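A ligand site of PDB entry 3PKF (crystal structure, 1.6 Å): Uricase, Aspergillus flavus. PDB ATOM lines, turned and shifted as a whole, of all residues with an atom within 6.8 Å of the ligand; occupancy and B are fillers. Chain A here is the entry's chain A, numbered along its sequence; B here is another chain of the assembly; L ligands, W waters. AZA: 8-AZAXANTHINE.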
ATOM      1  N   SER A 158      29.962  -8.028  -8.757  1.00  0.00           N
ATOM      2  CA  SER A 158      29.086  -9.167  -8.659  1.00  0.00           C
ATOM      3  C   SER A 158      28.211  -8.921  -7.439  1.00  0.00           C
ATOM      4  O   SER A 158      28.706  -8.460  -6.403  1.00  0.00           O
ATOM      5  CB  SER A 158      29.902 -10.468  -8.486  1.00  0.00           C
ATOM      6  OG  SER A 158      29.045 -11.561  -8.182  1.00  0.00           O
ATOM      7  N   GLN A 159      26.925  -9.209  -7.577  1.00  0.00           N
ATOM      8  CA  GLN A 159      25.943  -9.025  -6.524  1.00  0.00           C
ATOM      9  C   GLN A 159      25.111 -10.284  -6.372  1.00  0.00           C
ATOM     10  O   GLN A 159      25.024 -11.112  -7.306  1.00  0.00           O
ATOM     11  CB  GLN A 159      24.978  -7.856  -6.875  1.00  0.00           C
ATOM     12  CG  GLN A 159      25.730  -6.571  -7.201  1.00  0.00           C
ATOM     13  CD  GLN A 159      24.815  -5.389  -7.459  1.00  0.00           C
ATOM     14  OE1 GLN A 159      23.591  -5.474  -7.343  1.00  0.00           O
ATOM     15  NE2 GLN A 159      25.425  -4.257  -7.826  1.00  0.00           N
ATOM     16  N   PHE A 160      24.479 -10.433  -5.224  1.00  0.00           N
ATOM     17  CA  PHE A 160      23.495 -11.490  -5.075  1.00  0.00           C
ATOM     18  C   PHE A 160      22.523 -11.152  -3.952  1.00  0.00           C
ATOM     19  O   PHE A 160      22.809 -11.320  -2.777  1.00  0.00           O
ATOM     20  CB  PHE A 160      24.150 -12.896  -4.895  1.00  0.00           C
ATOM     21  CG  PHE A 160      23.171 -14.030  -5.028  1.00  0.00           C
ATOM     22  CD1 PHE A 160      22.522 -14.256  -6.240  1.00  0.00           C
ATOM     23  CD2 PHE A 160      22.869 -14.854  -3.940  1.00  0.00           C
ATOM     24  CE1 PHE A 160      21.584 -15.265  -6.374  1.00  0.00           C
ATOM     25  CE2 PHE A 160      21.941 -15.885  -4.066  1.00  0.00           C
ATOM     26  CZ  PHE A 160      21.269 -16.085  -5.284  1.00  0.00           C
ATOM     27  N   PHE A 163      16.988 -13.167  -3.267  1.00  0.00           N
ATOM     28  CA  PHE A 163      16.646 -14.586  -3.299  1.00  0.00           C
ATOM     29  C   PHE A 163      15.619 -14.977  -2.229  1.00  0.00           C
ATOM     30  O   PHE A 163      15.357 -14.204  -1.294  1.00  0.00           O
ATOM     31  CB  PHE A 163      17.920 -15.457  -3.186  1.00  0.00           C
ATOM     32  CG  PHE A 163      18.805 -15.076  -2.046  1.00  0.00           C
ATOM     33  CD1 PHE A 163      19.803 -14.123  -2.217  1.00  0.00           C
ATOM     34  CD2 PHE A 163      18.653 -15.673  -0.783  1.00  0.00           C
ATOM     35  CE1 PHE A 163      20.626 -13.743  -1.173  1.00  0.00           C
ATOM     36  CE2 PHE A 163      19.483 -15.300   0.270  1.00  0.00           C
ATOM     37  CZ  PHE A 163      20.459 -14.333   0.074  1.00  0.00           C
ATOM     38  N   LEU A 171      22.082 -17.172   4.517  1.00  0.00           N
ATOM     39  CA  LEU A 171      22.910 -16.340   3.640  1.00  0.00           C
ATOM     40  C   LEU A 171      22.452 -14.866   3.649  1.00  0.00           C
ATOM     41  O   LEU A 171      21.265 -14.577   3.459  1.00  0.00           O
ATOM     42  CB  LEU A 171      22.832 -16.893   2.201  1.00  0.00           C
ATOM     43  CG  LEU A 171      23.690 -16.172   1.129  1.00  0.00           C
ATOM     44  CD1 LEU A 171      25.183 -16.352   1.405  1.00  0.00           C
ATOM     45  CD2 LEU A 171      23.352 -16.664  -0.270  1.00  0.00           C
ATOM     46  N   ARG A 177      30.531  -8.700  -4.143  1.00  0.00           N
ATOM     47  CA  ARG A 177      31.215  -9.943  -3.743  1.00  0.00           C
ATOM     48  C   ARG A 177      32.229 -10.345  -4.801  1.00  0.00           C
ATOM     49  O   ARG A 177      32.255  -9.799  -5.904  1.00  0.00           O
ATOM     50  CB  ARG A 177      30.204 -11.083  -3.545  1.00  0.00           C
ATOM     51  CG  ARG A 177      29.526 -11.503  -4.822  1.00  0.00           C
ATOM     52  CD  ARG A 177      28.551 -12.670  -4.578  1.00  0.00           C
ATOM     53  NE  ARG A 177      28.036 -13.137  -5.869  1.00  0.00           N
ATOM     54  CZ  ARG A 177      27.295 -14.223  -6.071  1.00  0.00           C
ATOM     55  NH1 ARG A 177      26.883 -15.002  -5.064  1.00  0.00           N
ATOM     56  NH2 ARG A 177      26.917 -14.500  -7.324  1.00  0.00           N
ATOM     57  N   LEU A 179      33.476 -13.101  -7.502  1.00  0.00           N
ATOM     58  CA  LEU A 179      32.906 -14.167  -8.316  1.00  0.00           C
ATOM     59  C   LEU A 179      34.045 -14.879  -9.043  1.00  0.00           C
ATOM     60  O   LEU A 179      34.838 -14.275  -9.759  1.00  0.00           O
ATOM     61  CB  LEU A 179      31.884 -13.605  -9.313  1.00  0.00           C
ATOM     62  CG  LEU A 179      31.219 -14.594 -10.265  1.00  0.00           C
ATOM     63  CD1 LEU A 179      30.480 -15.638  -9.476  1.00  0.00           C
ATOM     64  CD2 LEU A 179      30.244 -13.836 -11.187  1.00  0.00           C
ATOM     65  N   SER A 225      27.119  -8.326 -12.422  1.00  0.00           N
ATOM     66  CA  SER A 225      26.401  -9.581 -12.372  1.00  0.00           C
ATOM     67  C   SER A 225      25.348  -9.655 -11.272  1.00  0.00           C
ATOM     68  O   SER A 225      25.623  -9.426 -10.092  1.00  0.00           O
ATOM     69  CB  SER A 225      27.429 -10.717 -12.208  1.00  0.00           C
ATOM     70  OG  SER A 225      26.749 -11.945 -12.068  1.00  0.00           O
ATOM     71  N   ALA A 226      24.125 -10.019 -11.653  1.00  0.00           N
ATOM     72  CA  ALA A 226      23.049 -10.131 -10.712  1.00  0.00           C
ATOM     73  C   ALA A 226      23.034 -11.509 -10.071  1.00  0.00           C
ATOM     74  O   ALA A 226      22.399 -11.726  -9.028  1.00  0.00           O
ATOM     75  CB  ALA A 226      21.713  -9.858 -11.421  1.00  0.00           C
ATOM     76  N   SER A 227      23.744 -12.436 -10.717  1.00  0.00           N
ATOM     77  CA  SER A 227      23.816 -13.853 -10.291  1.00  0.00           C
ATOM     78  C   SER A 227      24.623 -14.586 -11.349  1.00  0.00           C
ATOM     79  O   SER A 227      24.794 -14.075 -12.457  1.00  0.00           O
ATOM     80  CB  SER A 227      22.435 -14.550 -10.175  1.00  0.00           C
ATOM     81  OG  SER A 227      21.782 -14.668 -11.448  1.00  0.00           O
ATOM     82  N   VAL A 228      25.089 -15.792 -11.021  1.00  0.00           N
ATOM     83  CA  VAL A 228      25.769 -16.592 -12.022  1.00  0.00           C
ATOM     84  C   VAL A 228      24.774 -16.902 -13.147  1.00  0.00           C
ATOM     85  O   VAL A 228      25.124 -16.842 -14.323  1.00  0.00           O
ATOM     86  CB  VAL A 228      26.335 -17.879 -11.375  1.00  0.00           C
ATOM     87  CG1 VAL A 228      26.849 -18.806 -12.440  1.00  0.00           C
ATOM     88  CG2 VAL A 228      27.444 -17.494 -10.393  1.00  0.00           C
ATOM     89  N   GLN A 229      23.544 -17.238 -12.747  1.00  0.00           N
ATOM     90  CA  GLN A 229      22.448 -17.560 -13.685  1.00  0.00           C
ATOM     91  C   GLN A 229      22.291 -16.452 -14.740  1.00  0.00           C
ATOM     92  O   GLN A 229      22.263 -16.737 -15.959  1.00  0.00           O
ATOM     93  CB  GLN A 229      21.116 -17.724 -12.912  1.00  0.00           C
ATOM     94  CG  GLN A 229      20.987 -19.027 -12.104  1.00  0.00           C
ATOM     95  CD  GLN A 229      21.545 -18.943 -10.693  1.00  0.00           C
ATOM     96  OE1 GLN A 229      22.458 -18.159 -10.393  1.00  0.00           O
ATOM     97  NE2 GLN A 229      21.022 -19.808  -9.819  1.00  0.00           N
ATOM     98  N   ASN A 255      30.357 -22.162  -8.562  1.00  0.00           N
ATOM     99  CA  ASN A 255      30.521 -20.896  -7.917  1.00  0.00           C
ATOM    100  C   ASN A 255      31.553 -21.163  -6.821  1.00  0.00           C
ATOM    101  O   ASN A 255      31.229 -21.798  -5.843  1.00  0.00           O
ATOM    102  CB  ASN A 255      29.151 -20.427  -7.378  1.00  0.00           C
ATOM    103  CG  ASN A 255      29.177 -18.993  -6.858  1.00  0.00           C
ATOM    104  OD1 ASN A 255      30.210 -18.315  -6.899  1.00  0.00           O
ATOM    105  ND2 ASN A 255      28.040 -18.551  -6.318  1.00  0.00           N
ATOM    106  N   HIS A 257      33.560 -20.283  -3.872  1.00  0.00           N
ATOM    107  CA  HIS A 257      33.308 -19.239  -2.874  1.00  0.00           C
ATOM    108  C   HIS A 257      34.561 -18.719  -2.209  1.00  0.00           C
ATOM    109  O   HIS A 257      35.458 -19.493  -1.874  1.00  0.00           O
ATOM    110  CB  HIS A 257      32.329 -19.759  -1.798  1.00  0.00           C
ATOM    111  CG  HIS A 257      31.073 -20.335  -2.362  1.00  0.00           C
ATOM    112  ND1 HIS A 257      30.145 -19.580  -3.033  1.00  0.00           N
ATOM    113  CD2 HIS A 257      30.620 -21.616  -2.391  1.00  0.00           C
ATOM    114  CE1 HIS A 257      29.138 -20.359  -3.414  1.00  0.00           C
ATOM    115  NE2 HIS A 257      29.403 -21.601  -3.045  1.00  0.00           N
ATOM    116  N   GLY A 287      28.751 -23.954  -5.212  1.00  0.00           N
ATOM    117  CA  GLY A 287      27.542 -23.875  -6.043  1.00  0.00           C
ATOM    118  C   GLY A 287      27.832 -24.495  -7.402  1.00  0.00           C
ATOM    119  O   GLY A 287      28.982 -24.531  -7.858  1.00  0.00           O
ATOM    120  N   ILE A 289      25.928 -24.379 -11.246  1.00  0.00           N
ATOM    121  CA  ILE A 289      24.812 -23.758 -11.962  1.00  0.00           C
ATOM    122  C   ILE A 289      24.897 -24.176 -13.417  1.00  0.00           C
ATOM    123  O   ILE A 289      25.959 -24.016 -14.031  1.00  0.00           O
ATOM    124  CB  ILE A 289      24.903 -22.195 -11.907  1.00  0.00           C
ATOM    125  CG1 ILE A 289      25.262 -21.672 -10.491  1.00  0.00           C
ATOM    126  CG2 ILE A 289      23.570 -21.582 -12.414  1.00  0.00           C
ATOM    127  CD1 ILE A 289      24.334 -22.050  -9.440  1.00  0.00           C
ATOM    128  N   TYR B   9      20.371 -26.278 -10.928  1.00  0.00           N
ATOM    129  CA  TYR B   9      21.408 -25.572 -10.167  1.00  0.00           C
ATOM    130  C   TYR B   9      21.320 -26.123  -8.740  1.00  0.00           C
ATOM    131  O   TYR B   9      20.287 -26.660  -8.336  1.00  0.00           O
ATOM    132  CB  TYR B   9      21.201 -24.043 -10.209  1.00  0.00           C
ATOM    133  CG  TYR B   9      20.186 -23.621  -9.196  1.00  0.00           C
ATOM    134  CD1 TYR B   9      18.833 -23.880  -9.387  1.00  0.00           C
ATOM    135  CD2 TYR B   9      20.589 -23.075  -7.971  1.00  0.00           C
ATOM    136  CE1 TYR B   9      17.896 -23.570  -8.405  1.00  0.00           C
ATOM    137  CE2 TYR B   9      19.665 -22.748  -6.995  1.00  0.00           C
ATOM    138  CZ  TYR B   9      18.320 -23.008  -7.222  1.00  0.00           C
ATOM    139  OH  TYR B   9      17.398 -22.737  -6.258  1.00  0.00           O
ATOM    140  N   GLY B  10      22.401 -25.988  -7.979  1.00  0.00           N
ATOM    141  CA  GLY B  10      22.397 -26.445  -6.602  1.00  0.00           C
ATOM    142  C   GLY B  10      23.774 -26.418  -5.978  1.00  0.00           C
ATOM    143  O   GLY B  10      24.577 -25.586  -6.308  1.00  0.00           O
ATOM    144  N   LYS B  11      24.033 -27.352  -5.068  1.00  0.00           N
ATOM    145  CA  LYS B  11      25.291 -27.341  -4.307  1.00  0.00           C
ATOM    146  C   LYS B  11      25.974 -28.678  -4.510  1.00  0.00           C
ATOM    147  O   LYS B  11      25.333 -29.729  -4.401  1.00  0.00           O
ATOM    148  CB  LYS B  11      25.020 -27.160  -2.811  1.00  0.00           C
ATOM    149  CG  LYS B  11      26.234 -26.631  -2.036  1.00  0.00           C
ATOM    150  CD  LYS B  11      26.591 -25.211  -2.514  1.00  0.00           C
ATOM    151  CE  LYS B  11      26.790 -24.251  -1.396  1.00  0.00           C
ATOM    152  NZ  LYS B  11      26.890 -22.852  -1.883  1.00  0.00           N
ATOM    153  N   ASN B  52      15.768 -13.068  -8.899  1.00  0.00           N
ATOM    154  CA  ASN B  52      16.275 -14.007  -7.894  1.00  0.00           C
ATOM    155  C   ASN B  52      15.203 -14.560  -6.955  1.00  0.00           C
ATOM    156  O   ASN B  52      15.487 -15.434  -6.149  1.00  0.00           O
ATOM    157  CB  ASN B  52      17.469 -13.414  -7.140  1.00  0.00           C
ATOM    158  CG  ASN B  52      18.697 -13.236  -8.021  1.00  0.00           C
ATOM    159  OD1 ASN B  52      18.840 -13.923  -9.033  1.00  0.00           O
ATOM    160  ND2 ASN B  52      19.585 -12.313  -7.647  1.00  0.00           N
ATOM    161  N   ILE B  55      14.899 -18.281  -6.677  1.00  0.00           N
ATOM    162  CA  ILE B  55      16.076 -19.048  -6.309  1.00  0.00           C
ATOM    163  C   ILE B  55      16.104 -19.416  -4.824  1.00  0.00           C
ATOM    164  O   ILE B  55      16.143 -18.539  -3.960  1.00  0.00           O
ATOM    165  CB  ILE B  55      17.383 -18.304  -6.656  1.00  0.00           C
ATOM    166  CG1 ILE B  55      17.521 -18.103  -8.171  1.00  0.00           C
ATOM    167  CG2 ILE B  55      18.630 -19.118  -6.131  1.00  0.00           C
ATOM    168  CD1 ILE B  55      18.709 -17.205  -8.548  1.00  0.00           C
ATOM    169  N   VAL B  56      16.071 -20.714  -4.548  1.00  0.00           N
ATOM    170  CA  VAL B  56      16.434 -21.236  -3.238  1.00  0.00           C
ATOM    171  C   VAL B  56      17.968 -21.194  -3.259  1.00  0.00           C
ATOM    172  O   VAL B  56      18.566 -21.901  -4.071  1.00  0.00           O
ATOM    173  CB  VAL B  56      15.895 -22.674  -3.052  1.00  0.00           C
ATOM    174  CG1 VAL B  56      16.388 -23.289  -1.726  1.00  0.00           C
ATOM    175  CG2 VAL B  56      14.355 -22.672  -3.114  1.00  0.00           C
ATOM    176  N   ALA B  57      18.581 -20.357  -2.406  1.00  0.00           N
ATOM    177  CA  ALA B  57      20.032 -20.173  -2.480  1.00  0.00           C
ATOM    178  C   ALA B  57      20.759 -21.522  -2.299  1.00  0.00           C
ATOM    179  O   ALA B  57      20.292 -22.384  -1.549  1.00  0.00           O
ATOM    180  CB  ALA B  57      20.529 -19.139  -1.443  1.00  0.00           C
ATOM    181  N   THR B  58      21.879 -21.689  -3.001  1.00  0.00           N
ATOM    182  CA  THR B  58      22.623 -22.936  -2.919  1.00  0.00           C
ATOM    183  C   THR B  58      23.133 -23.073  -1.491  1.00  0.00           C
ATOM    184  O   THR B  58      23.184 -24.193  -0.972  1.00  0.00           O
ATOM    185  CB  THR B  58      23.788 -22.994  -3.939  1.00  0.00           C
ATOM    186  OG1 THR B  58      24.763 -22.013  -3.614  1.00  0.00           O
ATOM    187  CG2 THR B  58      23.252 -22.744  -5.390  1.00  0.00           C
ATOM    188  N   ASP B  59      23.440 -21.947  -0.841  1.00  0.00           N
ATOM    189  CA  ASP B  59      23.814 -21.964   0.574  1.00  0.00           C
ATOM    190  C   ASP B  59      22.703 -22.583   1.455  1.00  0.00           C
ATOM    191  O   ASP B  59      22.997 -23.331   2.381  1.00  0.00           O
ATOM    192  CB  ASP B  59      24.165 -20.567   1.077  1.00  0.00           C
ATOM    193  CG  ASP B  59      24.775 -20.585   2.461  1.00  0.00           C
ATOM    194  OD1 ASP B  59      25.981 -20.890   2.577  1.00  0.00           O
ATOM    195  OD2 ASP B  59      24.041 -20.322   3.440  1.00  0.00           O
ATOM    196  N   SER B  60      21.440 -22.260   1.143  1.00  0.00           N
ATOM    197  CA  SER B  60      20.304 -22.873   1.858  1.00  0.00           C
ATOM    198  C   SER B  60      20.152 -24.350   1.579  1.00  0.00           C
ATOM    199  O   SER B  60      19.741 -25.107   2.453  1.00  0.00           O
ATOM    200  CB  SER B  60      18.991 -22.121   1.512  1.00  0.00           C
ATOM    201  OG  SER B  60      19.207 -20.722   1.694  1.00  0.00           O
HETATM  202  N1  AZA L   1      23.548 -18.039  -7.636  1.00  0.00           N
HETATM  203  C2  AZA L   1      24.561 -17.206  -7.281  1.00  0.00           C
HETATM  204  O2  AZA L   1      25.064 -16.488  -8.166  1.00  0.00           O
HETATM  205  N3  AZA L   1      25.052 -17.128  -5.996  1.00  0.00           N
HETATM  206  C4  AZA L   1      24.442 -17.893  -5.073  1.00  0.00           C
HETATM  207  C5  AZA L   1      23.370 -18.785  -5.389  1.00  0.00           C
HETATM  208  C6  AZA L   1      22.910 -18.831  -6.781  1.00  0.00           C
HETATM  209  O6  AZA L   1      21.998 -19.617  -7.122  1.00  0.00           O
HETATM  210  N7  AZA L   1      22.975 -19.437  -4.257  1.00  0.00           N
HETATM  211  N8  AZA L   1      23.829 -18.915  -3.264  1.00  0.00           N
HETATM  212  N9  AZA L   1      24.759 -17.957  -3.729  1.00  0.00           N
HETATM  213  O   HOH W   1      26.250 -20.808  -5.659  1.00  0.00           O
HETATM  214  O   HOH W   2      26.859 -17.061  -2.334  1.00  0.00           O
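Merely in contact with the ligand: Phe 160 (3.4 Å), Ala 57 of chain B (3.5 Å), Ile 55 of chain B (3.5 Å), Ser 227 (3.6 Å), Leu 171 (3.8 Å), Tyr 9 of chain B (3.8 Å) and Asp 59 of chain B (3.9 Å).
Hydrophobic or aromatic side chains that line the ligand: Phe 160, Leu 171, Val 228, Tyr 9 of chain B, Ile 55 of chain B and Ala 57 of chain B.
Within 4 Å of the ligand: Phe 160, Leu 171, Arg 177, Ser 227, Val 228, Gln 229, Asn 255, Tyr 9 of chain B, Ile 55 of chain B, Ala 57 of chain B, Thr 58 of chain B and Asp 59 of chain B.
Water W2 bridges N9 of the ligand and NH1 of Arg 177.
Water W1 bridges the side-chain hydroxyl (OG1) of Thr 58 of chain B (2.8 Å) and the side-chain amide nitrogen (ND2) of Asn 255 (3.0 Å).
The backbone NH of Arg 177 is in hydrogen-bond range of the backbone carbonyl oxygen of Ser 158 (2.9 Å).
O of Gly 287 is in hydrogen-bond range of N of Asn 255.
O of Asn 255 sits at hydrogen-bond distance from NE2 of His 257.
The backbone carbonyl oxygen of Ser 227 is in hydrogen-bond range of the side-chain hydroxyl of Ser 225 (2.9 Å).
OH of Tyr 9 of chain B is in hydrogen-bond range of O of Val 56 of chain B, 2.6 Å away.
The side-chain hydroxyl (OG) of Ser 227 lies close to the backbone NH (N) of Gln 229.
The side-chain hydroxyl (OG1) of Thr 58 of chain B sits at hydrogen-bond distance from the side-chain amino group (NZ) of Lys 11 of chain B, 2.9 Å away.
A nitrogen (N7) of the ligand sits at hydrogen-bond distance from the backbone NH of Thr 58 of chain B (2.8 Å).
NH2 of Arg 177 is in hydrogen-bond range of O2 of the ligand, 2.8 Å away.
NE2 of Gln 229 lies within hydrogen-bond range of O6 of the ligand (2.9 Å).
N7 of the ligand lies within hydrogen-bond range of OG1 of Thr 58 of chain B (3.2 Å).
N of Val 228 sits at hydrogen-bond distance from O2 of the ligand, 2.9 Å away.
ND2 of Asn 255 sits close to N3 of the ligand, at 3.3 Å.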
